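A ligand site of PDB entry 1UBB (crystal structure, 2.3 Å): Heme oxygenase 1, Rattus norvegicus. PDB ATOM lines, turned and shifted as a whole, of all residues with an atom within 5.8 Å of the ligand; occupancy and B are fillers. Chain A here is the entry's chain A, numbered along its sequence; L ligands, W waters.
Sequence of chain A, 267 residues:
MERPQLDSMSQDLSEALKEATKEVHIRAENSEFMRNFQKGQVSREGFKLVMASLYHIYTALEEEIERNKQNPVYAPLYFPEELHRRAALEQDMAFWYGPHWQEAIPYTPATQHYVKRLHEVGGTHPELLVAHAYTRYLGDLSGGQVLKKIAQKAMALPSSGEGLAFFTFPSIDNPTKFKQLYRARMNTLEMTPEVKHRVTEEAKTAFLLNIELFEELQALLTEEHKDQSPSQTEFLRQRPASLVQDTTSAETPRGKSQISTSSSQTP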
ATOM      1  N   SER A  14     -40.499   1.619 -24.971  1.00  0.00           N
ATOM      2  CA  SER A  14     -39.112   2.043 -24.895  1.00  0.00           C
ATOM      3  C   SER A  14     -38.991   3.352 -24.117  1.00  0.00           C
ATOM      4  O   SER A  14     -38.137   3.497 -23.249  1.00  0.00           O
ATOM      5  CB  SER A  14     -38.524   2.225 -26.303  1.00  0.00           C
ATOM      6  OG  SER A  14     -39.254   3.190 -27.049  1.00  0.00           O
ATOM      7  N   LEU A  17     -39.930   2.974 -20.407  1.00  0.00           N
ATOM      8  CA  LEU A  17     -38.846   2.362 -19.646  1.00  0.00           C
ATOM      9  C   LEU A  17     -37.704   3.325 -19.358  1.00  0.00           C
ATOM     10  O   LEU A  17     -37.159   3.321 -18.254  1.00  0.00           O
ATOM     11  CB  LEU A  17     -38.307   1.131 -20.392  1.00  0.00           C
ATOM     12  CG  LEU A  17     -39.085  -0.162 -20.185  1.00  0.00           C
ATOM     13  CD1 LEU A  17     -38.663  -1.221 -21.175  1.00  0.00           C
ATOM     14  CD2 LEU A  17     -38.842  -0.651 -18.766  1.00  0.00           C
ATOM     15  N   LYS A  18     -37.346   4.146 -20.338  1.00  0.00           N
ATOM     16  CA  LYS A  18     -36.262   5.100 -20.148  1.00  0.00           C
ATOM     17  C   LYS A  18     -36.684   6.117 -19.093  1.00  0.00           C
ATOM     18  O   LYS A  18     -35.893   6.483 -18.218  1.00  0.00           O
ATOM     19  CB  LYS A  18     -35.942   5.824 -21.462  1.00  0.00           C
ATOM     20  CG  LYS A  18     -34.770   6.787 -21.336  1.00  0.00           C
ATOM     21  CD  LYS A  18     -34.547   7.552 -22.630  1.00  0.00           C
ATOM     22  CE  LYS A  18     -33.360   8.509 -22.497  1.00  0.00           C
ATOM     23  NZ  LYS A  18     -33.176   9.356 -23.715  1.00  0.00           N
ATOM     24  N   THR A  21     -36.780   4.453 -15.476  1.00  0.00           N
ATOM     25  CA  THR A  21     -35.538   4.065 -14.848  1.00  0.00           C
ATOM     26  C   THR A  21     -34.449   5.136 -14.845  1.00  0.00           C
ATOM     27  O   THR A  21     -33.360   4.907 -14.336  1.00  0.00           O
ATOM     28  CB  THR A  21     -34.971   2.811 -15.525  1.00  0.00           C
ATOM     29  OG1 THR A  21     -34.693   3.098 -16.895  1.00  0.00           O
ATOM     30  CG2 THR A  21     -35.982   1.661 -15.427  1.00  0.00           C
ATOM     31  N   HIS A  25     -31.231   5.002 -12.546  1.00  0.00           N
ATOM     32  CA  HIS A  25     -30.039   4.789 -13.349  1.00  0.00           C
ATOM     33  C   HIS A  25     -28.949   5.702 -12.804  1.00  0.00           C
ATOM     34  O   HIS A  25     -27.773   5.323 -12.708  1.00  0.00           O
ATOM     35  CB  HIS A  25     -30.287   5.117 -14.826  1.00  0.00           C
ATOM     36  CG  HIS A  25     -29.083   4.918 -15.685  1.00  0.00           C
ATOM     37  ND1 HIS A  25     -27.968   5.724 -15.603  1.00  0.00           N
ATOM     38  CD2 HIS A  25     -28.806   3.978 -16.616  1.00  0.00           C
ATOM     39  CE1 HIS A  25     -27.052   5.288 -16.451  1.00  0.00           C
ATOM     40  NE2 HIS A  25     -27.532   4.225 -17.076  1.00  0.00           N
ATOM     41  N   ALA A  28     -27.602   4.269  -9.720  1.00  0.00           N
ATOM     42  CA  ALA A  28     -26.841   3.071 -10.069  1.00  0.00           C
ATOM     43  C   ALA A  28     -25.442   3.383 -10.587  1.00  0.00           C
ATOM     44  O   ALA A  28     -24.464   2.788 -10.142  1.00  0.00           O
ATOM     45  CB  ALA A  28     -27.596   2.242 -11.110  1.00  0.00           C
ATOM     46  N   GLU A  29     -25.339   4.318 -11.522  1.00  0.00           N
ATOM     47  CA  GLU A  29     -24.024   4.664 -12.063  1.00  0.00           C
ATOM     48  C   GLU A  29     -23.192   5.446 -11.079  1.00  0.00           C
ATOM     49  O   GLU A  29     -21.998   5.677 -11.300  1.00  0.00           O
ATOM     50  CB  GLU A  29     -24.169   5.440 -13.367  1.00  0.00           C
ATOM     51  CG  GLU A  29     -24.772   6.809 -13.218  1.00  0.00           C
ATOM     52  CD  GLU A  29     -24.862   7.529 -14.552  1.00  0.00           C
ATOM     53  OE1 GLU A  29     -23.806   7.713 -15.199  1.00  0.00           O
ATOM     54  OE2 GLU A  29     -25.988   7.904 -14.940  1.00  0.00           O
ATOM     55  N   MET A  34     -19.168   1.603  -8.696  1.00  0.00           N
ATOM     56  CA  MET A  34     -19.037   2.167 -10.020  1.00  0.00           C
ATOM     57  C   MET A  34     -18.207   3.446 -10.021  1.00  0.00           C
ATOM     58  O   MET A  34     -17.525   3.744 -10.998  1.00  0.00           O
ATOM     59  CB  MET A  34     -20.411   2.457 -10.649  1.00  0.00           C
ATOM     60  CG  MET A  34     -21.240   1.210 -10.992  1.00  0.00           C
ATOM     61  SD  MET A  34     -20.427  -0.043 -12.033  1.00  0.00           S
ATOM     62  CE  MET A  34     -19.133   0.889 -12.826  1.00  0.00           C
ATOM     63  N   GLN A  38     -15.054   3.843 -12.277  1.00  0.00           N
ATOM     64  CA  GLN A  38     -14.911   4.929 -13.236  1.00  0.00           C
ATOM     65  C   GLN A  38     -13.672   5.777 -12.973  1.00  0.00           C
ATOM     66  O   GLN A  38     -13.167   6.417 -13.892  1.00  0.00           O
ATOM     67  CB  GLN A  38     -16.145   5.827 -13.217  1.00  0.00           C
ATOM     68  CG  GLN A  38     -17.436   5.120 -13.604  1.00  0.00           C
ATOM     69  CD  GLN A  38     -18.603   6.083 -13.732  1.00  0.00           C
ATOM     70  OE1 GLN A  38     -18.649   6.893 -14.650  1.00  0.00           O
ATOM     71  NE2 GLN A  38     -19.541   5.993 -12.791  1.00  0.00           N
ATOM     72  N   TYR A 114     -30.599 -11.935  -6.995  1.00  0.00           N
ATOM     73  CA  TYR A 114     -30.860 -11.474  -8.356  1.00  0.00           C
ATOM     74  C   TYR A 114     -31.289 -12.667  -9.231  1.00  0.00           C
ATOM     75  O   TYR A 114     -32.268 -12.590  -9.962  1.00  0.00           O
ATOM     76  CB  TYR A 114     -29.581 -10.844  -8.913  1.00  0.00           C
ATOM     77  CG  TYR A 114     -29.748  -9.906 -10.101  1.00  0.00           C
ATOM     78  CD1 TYR A 114     -30.744 -10.099 -11.063  1.00  0.00           C
ATOM     79  CD2 TYR A 114     -28.848  -8.857 -10.286  1.00  0.00           C
ATOM     80  CE1 TYR A 114     -30.818  -9.288 -12.191  1.00  0.00           C
ATOM     81  CE2 TYR A 114     -28.907  -8.041 -11.398  1.00  0.00           C
ATOM     82  CZ  TYR A 114     -29.894  -8.252 -12.350  1.00  0.00           C
ATOM     83  OH  TYR A 114     -29.927  -7.448 -13.457  1.00  0.00           O
ATOM     84  N   TYR A 134     -33.748  -5.783 -21.109  1.00  0.00           N
ATOM     85  CA  TYR A 134     -33.551  -4.362 -21.396  1.00  0.00           C
ATOM     86  C   TYR A 134     -32.498  -3.778 -20.452  1.00  0.00           C
ATOM     87  O   TYR A 134     -31.511  -3.196 -20.898  1.00  0.00           O
ATOM     88  CB  TYR A 134     -34.873  -3.610 -21.208  1.00  0.00           C
ATOM     89  CG  TYR A 134     -34.743  -2.117 -20.987  1.00  0.00           C
ATOM     90  CD1 TYR A 134     -34.523  -1.248 -22.050  1.00  0.00           C
ATOM     91  CD2 TYR A 134     -34.867  -1.590 -19.707  1.00  0.00           C
ATOM     92  CE1 TYR A 134     -34.435   0.136 -21.840  1.00  0.00           C
ATOM     93  CE2 TYR A 134     -34.782  -0.218 -19.485  1.00  0.00           C
ATOM     94  CZ  TYR A 134     -34.568   0.639 -20.545  1.00  0.00           C
ATOM     95  OH  TYR A 134     -34.520   1.998 -20.313  1.00  0.00           O
ATOM     96  N   THR A 135     -32.717  -3.950 -19.159  1.00  0.00           N
ATOM     97  CA  THR A 135     -31.815  -3.430 -18.129  1.00  0.00           C
ATOM     98  C   THR A 135     -30.363  -3.872 -18.295  1.00  0.00           C
ATOM     99  O   THR A 135     -29.444  -3.049 -18.227  1.00  0.00           O
ATOM    100  CB  THR A 135     -32.319  -3.826 -16.724  1.00  0.00           C
ATOM    101  OG1 THR A 135     -33.547  -3.148 -16.449  1.00  0.00           O
ATOM    102  CG2 THR A 135     -31.277  -3.480 -15.642  1.00  0.00           C
ATOM    103  N   ARG A 136     -30.137  -5.169 -18.489  1.00  0.00           N
ATOM    104  CA  ARG A 136     -28.776  -5.674 -18.626  1.00  0.00           C
ATOM    105  C   ARG A 136     -28.141  -5.370 -19.994  1.00  0.00           C
ATOM    106  O   ARG A 136     -27.120  -4.703 -20.063  1.00  0.00           O
ATOM    107  CB  ARG A 136     -28.744  -7.186 -18.379  1.00  0.00           C
ATOM    108  CG  ARG A 136     -28.932  -7.643 -16.935  1.00  0.00           C
ATOM    109  CD  ARG A 136     -27.914  -7.030 -15.963  1.00  0.00           C
ATOM    110  NE  ARG A 136     -26.609  -6.750 -16.579  1.00  0.00           N
ATOM    111  CZ  ARG A 136     -25.634  -6.067 -15.985  1.00  0.00           C
ATOM    112  NH1 ARG A 136     -24.486  -5.852 -16.617  1.00  0.00           N
ATOM    113  NH2 ARG A 136     -25.795  -5.606 -14.762  1.00  0.00           N
ATOM    114  N   LEU A 138     -29.008  -3.371 -22.743  1.00  0.00           N
ATOM    115  CA  LEU A 138     -28.802  -2.010 -23.223  1.00  0.00           C
ATOM    116  C   LEU A 138     -27.781  -1.269 -22.357  1.00  0.00           C
ATOM    117  O   LEU A 138     -27.181  -0.291 -22.801  1.00  0.00           O
ATOM    118  CB  LEU A 138     -30.129  -1.239 -23.263  1.00  0.00           C
ATOM    119  CG  LEU A 138     -31.131  -1.624 -24.362  1.00  0.00           C
ATOM    120  CD1 LEU A 138     -31.714  -0.355 -24.955  1.00  0.00           C
ATOM    121  CD2 LEU A 138     -30.470  -2.443 -25.454  1.00  0.00           C
ATOM    122  N   GLY A 139     -27.600  -1.737 -21.130  1.00  0.00           N
ATOM    123  CA  GLY A 139     -26.609  -1.122 -20.255  1.00  0.00           C
ATOM    124  C   GLY A 139     -25.251  -1.565 -20.749  1.00  0.00           C
ATOM    125  O   GLY A 139     -24.287  -0.789 -20.771  1.00  0.00           O
ATOM    126  N   ASP A 140     -25.177  -2.840 -21.144  1.00  0.00           N
ATOM    127  CA  ASP A 140     -23.930  -3.394 -21.662  1.00  0.00           C
ATOM    128  C   ASP A 140     -23.516  -2.627 -22.900  1.00  0.00           C
ATOM    129  O   ASP A 140     -22.338  -2.318 -23.082  1.00  0.00           O
ATOM    130  CB  ASP A 140     -24.104  -4.870 -22.018  1.00  0.00           C
ATOM    131  CG  ASP A 140     -24.348  -5.737 -20.804  1.00  0.00           C
ATOM    132  OD1 ASP A 140     -23.796  -5.411 -19.740  1.00  0.00           O
ATOM    133  OD2 ASP A 140     -25.066  -6.745 -20.928  1.00  0.00           O
ATOM    134  N   SER A 142     -24.120   0.380 -23.545  1.00  0.00           N
ATOM    135  CA  SER A 142     -23.956   1.801 -23.255  1.00  0.00           C
ATOM    136  C   SER A 142     -22.833   2.016 -22.244  1.00  0.00           C
ATOM    137  O   SER A 142     -21.681   2.211 -22.616  1.00  0.00           O
ATOM    138  CB  SER A 142     -25.267   2.375 -22.743  1.00  0.00           C
ATOM    139  OG  SER A 142     -26.327   2.097 -23.650  1.00  0.00           O
ATOM    140  N   GLY A 143     -23.176   1.971 -20.962  1.00  0.00           N
ATOM    141  CA  GLY A 143     -22.179   2.164 -19.917  1.00  0.00           C
ATOM    142  C   GLY A 143     -21.097   1.098 -19.904  1.00  0.00           C
ATOM    143  O   GLY A 143     -19.938   1.390 -19.634  1.00  0.00           O
ATOM    144  N   GLY A 144     -21.474  -0.141 -20.187  1.00  0.00           N
ATOM    145  CA  GLY A 144     -20.501  -1.214 -20.218  1.00  0.00           C
ATOM    146  C   GLY A 144     -19.338  -0.919 -21.161  1.00  0.00           C
ATOM    147  O   GLY A 144     -18.195  -1.267 -20.873  1.00  0.00           O
ATOM    148  N   VAL A 146     -18.102   1.980 -21.861  1.00  0.00           N
ATOM    149  CA  VAL A 146     -17.263   2.997 -21.262  1.00  0.00           C
ATOM    150  C   VAL A 146     -16.394   2.332 -20.203  1.00  0.00           C
ATOM    151  O   VAL A 146     -15.209   2.644 -20.087  1.00  0.00           O
ATOM    152  CB  VAL A 146     -18.115   4.110 -20.603  1.00  0.00           C
ATOM    153  CG1 VAL A 146     -17.221   5.051 -19.824  1.00  0.00           C
ATOM    154  CG2 VAL A 146     -18.882   4.873 -21.685  1.00  0.00           C
ATOM    155  N   LEU A 147     -16.980   1.412 -19.447  1.00  0.00           N
ATOM    156  CA  LEU A 147     -16.235   0.704 -18.415  1.00  0.00           C
ATOM    157  C   LEU A 147     -15.167  -0.176 -19.035  1.00  0.00           C
ATOM    158  O   LEU A 147     -14.123  -0.399 -18.443  1.00  0.00           O
ATOM    159  CB  LEU A 147     -17.169  -0.146 -17.565  1.00  0.00           C
ATOM    160  CG  LEU A 147     -18.184   0.594 -16.698  1.00  0.00           C
ATOM    161  CD1 LEU A 147     -18.887  -0.409 -15.800  1.00  0.00           C
ATOM    162  CD2 LEU A 147     -17.465   1.654 -15.854  1.00  0.00           C
ATOM    163  N   LYS A 179     -29.185  -0.612 -30.620  1.00  0.00           N
ATOM    164  CA  LYS A 179     -30.065  -0.186 -29.542  1.00  0.00           C
ATOM    165  C   LYS A 179     -31.343   0.412 -30.118  1.00  0.00           C
ATOM    166  O   LYS A 179     -32.432   0.185 -29.603  1.00  0.00           O
ATOM    167  CB  LYS A 179     -29.339   0.813 -28.633  1.00  0.00           C
ATOM    168  CG  LYS A 179     -28.464   0.151 -27.587  1.00  0.00           C
ATOM    169  CD  LYS A 179     -27.146   0.888 -27.375  1.00  0.00           C
ATOM    170  CE  LYS A 179     -27.362   2.326 -26.937  1.00  0.00           C
ATOM    171  NZ  LYS A 179     -26.070   3.033 -26.737  1.00  0.00           N
ATOM    172  N   ARG A 183     -35.003  -0.888 -29.311  1.00  0.00           N
ATOM    173  CA  ARG A 183     -36.055  -0.055 -28.732  1.00  0.00           C
ATOM    174  C   ARG A 183     -37.317  -0.160 -29.562  1.00  0.00           C
ATOM    175  O   ARG A 183     -38.410  -0.303 -29.033  1.00  0.00           O
ATOM    176  CB  ARG A 183     -35.618   1.417 -28.650  1.00  0.00           C
ATOM    177  CG  ARG A 183     -34.457   1.688 -27.706  1.00  0.00           C
ATOM    178  CD  ARG A 183     -34.256   3.184 -27.462  1.00  0.00           C
ATOM    179  NE  ARG A 183     -33.098   3.422 -26.607  1.00  0.00           N
ATOM    180  CZ  ARG A 183     -31.857   3.563 -27.039  1.00  0.00           C
ATOM    181  NH1 ARG A 183     -31.583   3.510 -28.336  1.00  0.00           N
ATOM    182  NH2 ARG A 183     -30.859   3.736 -26.169  1.00  0.00           N
ATOM    183  N   PHE A 207     -32.784  -2.700 -11.722  1.00  0.00           N
ATOM    184  CA  PHE A 207     -31.752  -1.743 -11.364  1.00  0.00           C
ATOM    185  C   PHE A 207     -31.381  -1.861  -9.894  1.00  0.00           C
ATOM    186  O   PHE A 207     -30.196  -1.835  -9.546  1.00  0.00           O
ATOM    187  CB  PHE A 207     -32.216  -0.317 -11.659  1.00  0.00           C
ATOM    188  CG  PHE A 207     -31.875   0.161 -13.040  1.00  0.00           C
ATOM    189  CD1 PHE A 207     -32.741  -0.051 -14.106  1.00  0.00           C
ATOM    190  CD2 PHE A 207     -30.673   0.828 -13.280  1.00  0.00           C
ATOM    191  CE1 PHE A 207     -32.426   0.397 -15.385  1.00  0.00           C
ATOM    192  CE2 PHE A 207     -30.344   1.280 -14.541  1.00  0.00           C
ATOM    193  CZ  PHE A 207     -31.224   1.053 -15.602  1.00  0.00           C
ATOM    194  N   ASN A 210     -29.234  -4.677  -9.058  1.00  0.00           N
ATOM    195  CA  ASN A 210     -27.880  -4.349  -9.483  1.00  0.00           C
ATOM    196  C   ASN A 210     -27.219  -3.446  -8.456  1.00  0.00           C
ATOM    197  O   ASN A 210     -26.069  -3.654  -8.089  1.00  0.00           O
ATOM    198  CB  ASN A 210     -27.905  -3.648 -10.842  1.00  0.00           C
ATOM    199  CG  ASN A 210     -27.901  -4.639 -11.990  1.00  0.00           C
ATOM    200  OD1 ASN A 210     -26.876  -5.239 -12.303  1.00  0.00           O
ATOM    201  ND2 ASN A 210     -29.058  -4.824 -12.622  1.00  0.00           N
ATOM    202  N   PHE A 214     -23.790  -4.248  -6.184  1.00  0.00           N
ATOM    203  CA  PHE A 214     -22.639  -3.366  -6.077  1.00  0.00           C
ATOM    204  C   PHE A 214     -22.330  -2.986  -4.646  1.00  0.00           C
ATOM    205  O   PHE A 214     -21.166  -2.978  -4.239  1.00  0.00           O
ATOM    206  CB  PHE A 214     -22.852  -2.096  -6.909  1.00  0.00           C
ATOM    207  CG  PHE A 214     -22.975  -2.359  -8.388  1.00  0.00           C
ATOM    208  CD1 PHE A 214     -22.210  -3.364  -8.993  1.00  0.00           C
ATOM    209  CD2 PHE A 214     -23.855  -1.624  -9.170  1.00  0.00           C
ATOM    210  CE1 PHE A 214     -22.332  -3.627 -10.358  1.00  0.00           C
ATOM    211  CE2 PHE A 214     -23.980  -1.877 -10.535  1.00  0.00           C
ATOM    212  CZ  PHE A 214     -23.222  -2.885 -11.127  1.00  0.00           C
HETATM  213  C1  LIG L   1     -28.183   3.900 -21.066  1.00  0.00           C
HETATM  214  C2  LIG L   1     -24.047   5.466 -19.147  1.00  0.00           C
HETATM  215  C3  LIG L   1     -24.456   2.119 -15.657  1.00  0.00           C
HETATM  216  C4  LIG L   1     -28.353   0.317 -17.792  1.00  0.00           C
HETATM  217  C5  LIG L   1     -27.025   4.656 -20.856  1.00  0.00           C
HETATM  218  C6  LIG L   1     -26.592   5.778 -21.674  1.00  0.00           C
HETATM  219  C7  LIG L   1     -25.356   6.139 -21.202  1.00  0.00           C
HETATM  220  C8  LIG L   1     -25.132   5.337 -19.999  1.00  0.00           C
HETATM  221  C9  LIG L   1     -24.392   7.158 -21.743  1.00  0.00           C
HETATM  222  C10 LIG L   1     -27.385   6.395 -22.831  1.00  0.00           C
HETATM  223  C11 LIG L   1     -27.187   5.714 -24.230  1.00  0.00           C
HETATM  224  C12 LIG L   1     -28.261   5.832 -25.168  1.00  0.00           C
HETATM  225  O1  LIG L   1     -28.265   4.954 -26.127  1.00  0.00           O
HETATM  226  O2  LIG L   1     -29.168   6.705 -25.106  1.00  0.00           O
HETATM  227  C13 LIG L   1     -23.735   4.600 -18.096  1.00  0.00           C
HETATM  228  C14 LIG L   1     -22.482   4.627 -17.351  1.00  0.00           C
HETATM  229  C15 LIG L   1     -22.650   3.786 -16.303  1.00  0.00           C
HETATM  230  C16 LIG L   1     -23.931   3.114 -16.499  1.00  0.00           C
HETATM  231  C17 LIG L   1     -21.285   5.483 -17.729  1.00  0.00           C
HETATM  232  C18 LIG L   1     -21.742   3.589 -15.119  1.00  0.00           C
HETATM  233  C19 LIG L   1     -20.915   2.309 -15.219  1.00  0.00           C
HETATM  234  C20 LIG L   1     -25.566   1.357 -15.899  1.00  0.00           C
HETATM  235  C21 LIG L   1     -26.019   0.250 -15.056  1.00  0.00           C
HETATM  236  C22 LIG L   1     -27.146  -0.211 -15.651  1.00  0.00           C
HETATM  237  C23 LIG L   1     -27.347   0.546 -16.867  1.00  0.00           C
HETATM  238  C24 LIG L   1     -25.324  -0.211 -13.785  1.00  0.00           C
HETATM  239  C25 LIG L   1     -28.127  -1.278 -15.112  1.00  0.00           C
HETATM  240  C26 LIG L   1     -27.478  -2.683 -14.990  1.00  0.00           C
HETATM  241  C27 LIG L   1     -28.720   1.186 -18.840  1.00  0.00           C
HETATM  242  C28 LIG L   1     -29.927   1.037 -19.649  1.00  0.00           C
HETATM  243  C29 LIG L   1     -29.820   1.994 -20.618  1.00  0.00           C
HETATM  244  C30 LIG L   1     -28.614   2.778 -20.320  1.00  0.00           C
HETATM  245  C31 LIG L   1     -31.005   0.021 -19.390  1.00  0.00           C
HETATM  246  C32 LIG L   1     -30.697   2.286 -21.808  1.00  0.00           C
HETATM  247  C33 LIG L   1     -31.753   3.435 -21.514  1.00  0.00           C
HETATM  248  C34 LIG L   1     -32.581   3.680 -22.629  1.00  0.00           C
HETATM  249  O3  LIG L   1     -33.788   3.298 -22.600  1.00  0.00           O
HETATM  250  O4  LIG L   1     -32.139   4.256 -23.651  1.00  0.00           O
HETATM  251  N1  LIG L   1     -26.147   4.418 -19.827  1.00  0.00           N
HETATM  252  N2  LIG L   1     -24.559   3.597 -17.623  1.00  0.00           N
HETATM  253  N3  LIG L   1     -26.425   1.550 -16.992  1.00  0.00           N
HETATM  254  N4  LIG L   1     -27.980   2.276 -19.237  1.00  0.00           N
HETATM  255 FE1  LIG L   1     -26.295   2.981 -18.350  1.00  0.00          FE
HETATM  256  O   HOH W   1     -26.563  -2.959 -17.923  1.00  0.00           O
HETATM  257  O   HOH W   2     -35.566   3.344 -24.522  1.00  0.00           O
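The side-chain amino group (NZ) of Lys 179 sits at hydrogen-bond distance from the side-chain hydroxyl (OG) of Ser 142 (3.2 Å). OG of Ser 142 lies within hydrogen-bond range of O of Leu 138 (2.7 Å). The backbone carbonyl oxygen of Gly 139 is in hydrogen-bond range of the backbone NH of Gly 144, 2.9 Å away. A ring nitrogen (ND1) of His 25 lies within hydrogen-bond range of the side-chain carboxylate (OE2) of Glu 29. The side-chain amide oxygen of Asn 210 lies within hydrogen-bond range of the guanidinium group of Arg 136, at 2.7 Å. The side-chain amide nitrogen (ND2) of Asn 210 is in hydrogen-bond range of the side-chain hydroxyl (OH) of Tyr 114, 2.9 Å away. NH1 of Arg 136 lies within salt-bridge range of OD1 of Asp 140. The backbone carbonyl oxygen of Glu 29 is in hydrogen-bond range of the side-chain amide nitrogen of Gln 38, at 2.9 Å.
Lys 18 touches the ligand (CB to O3, 3.5 Å). CB of Glu 29 touches C18 of the ligand, at 3.5 Å. Met 34 touches the ligand (CE to C19, 3.3 Å). Thr 135 touches the ligand. NH2 of Arg 136 touches C26 of the ligand, 3.4 Å away. CB of Leu 138 touches C32 of the ligand, 3.9 Å away. Gly 139 touches the ligand (CA to C4, 3.3 Å). Ser 142 touches the ligand (CB to C5, 3.4 Å). CA of Gly 143 touches C13 of the ligand (3.4 Å). Leu 147 touches the ligand (CD1 to C19, 3.4 Å). Phe 207 touches the ligand. Asn 210 touches the ligand (ND2 to C26, 3.6 Å). Phe 214 touches the ligand (CE2 to C24, 3.9 Å). Hydrophobic or aromatic side chains that line the ligand: His 25, Met 34, Tyr 134, Leu 138, Leu 147, Phe 207 and Phe 214. Within 4 Å of the ligand: Lys 18, His 25, Glu 29, Met 34, Tyr 134, Thr 135, Arg 136, Leu 138, Gly 139, Ser 142, Gly 143, Leu 147, Lys 179, Arg 183, Phe 207, Asn 210 and Phe 214. Along chain A the residues within 4 Å of the ligand span positions 18 to 214.
Water W2 lies within hydrogen-bond range of an oxygen (O3) of the ligand (2.6 Å), the backbone carbonyl oxygen of Ser 14 (2.9 Å) and the guanidinium group of Arg 183 (3.2 Å).
A ring nitrogen (NE2) of His 25 is bound to an iron atom (FE1) of the ligand. An oxygen (O1) of the ligand lies within salt-bridge range of the guanidinium group (NH2) of Arg 183, 2.9 Å away. O1 of the ligand is in salt-bridge range of NZ of Lys 179, at 3.0 Å. An oxygen (O3) of the ligand is in hydrogen-bond range of the side-chain hydroxyl of Tyr 134.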
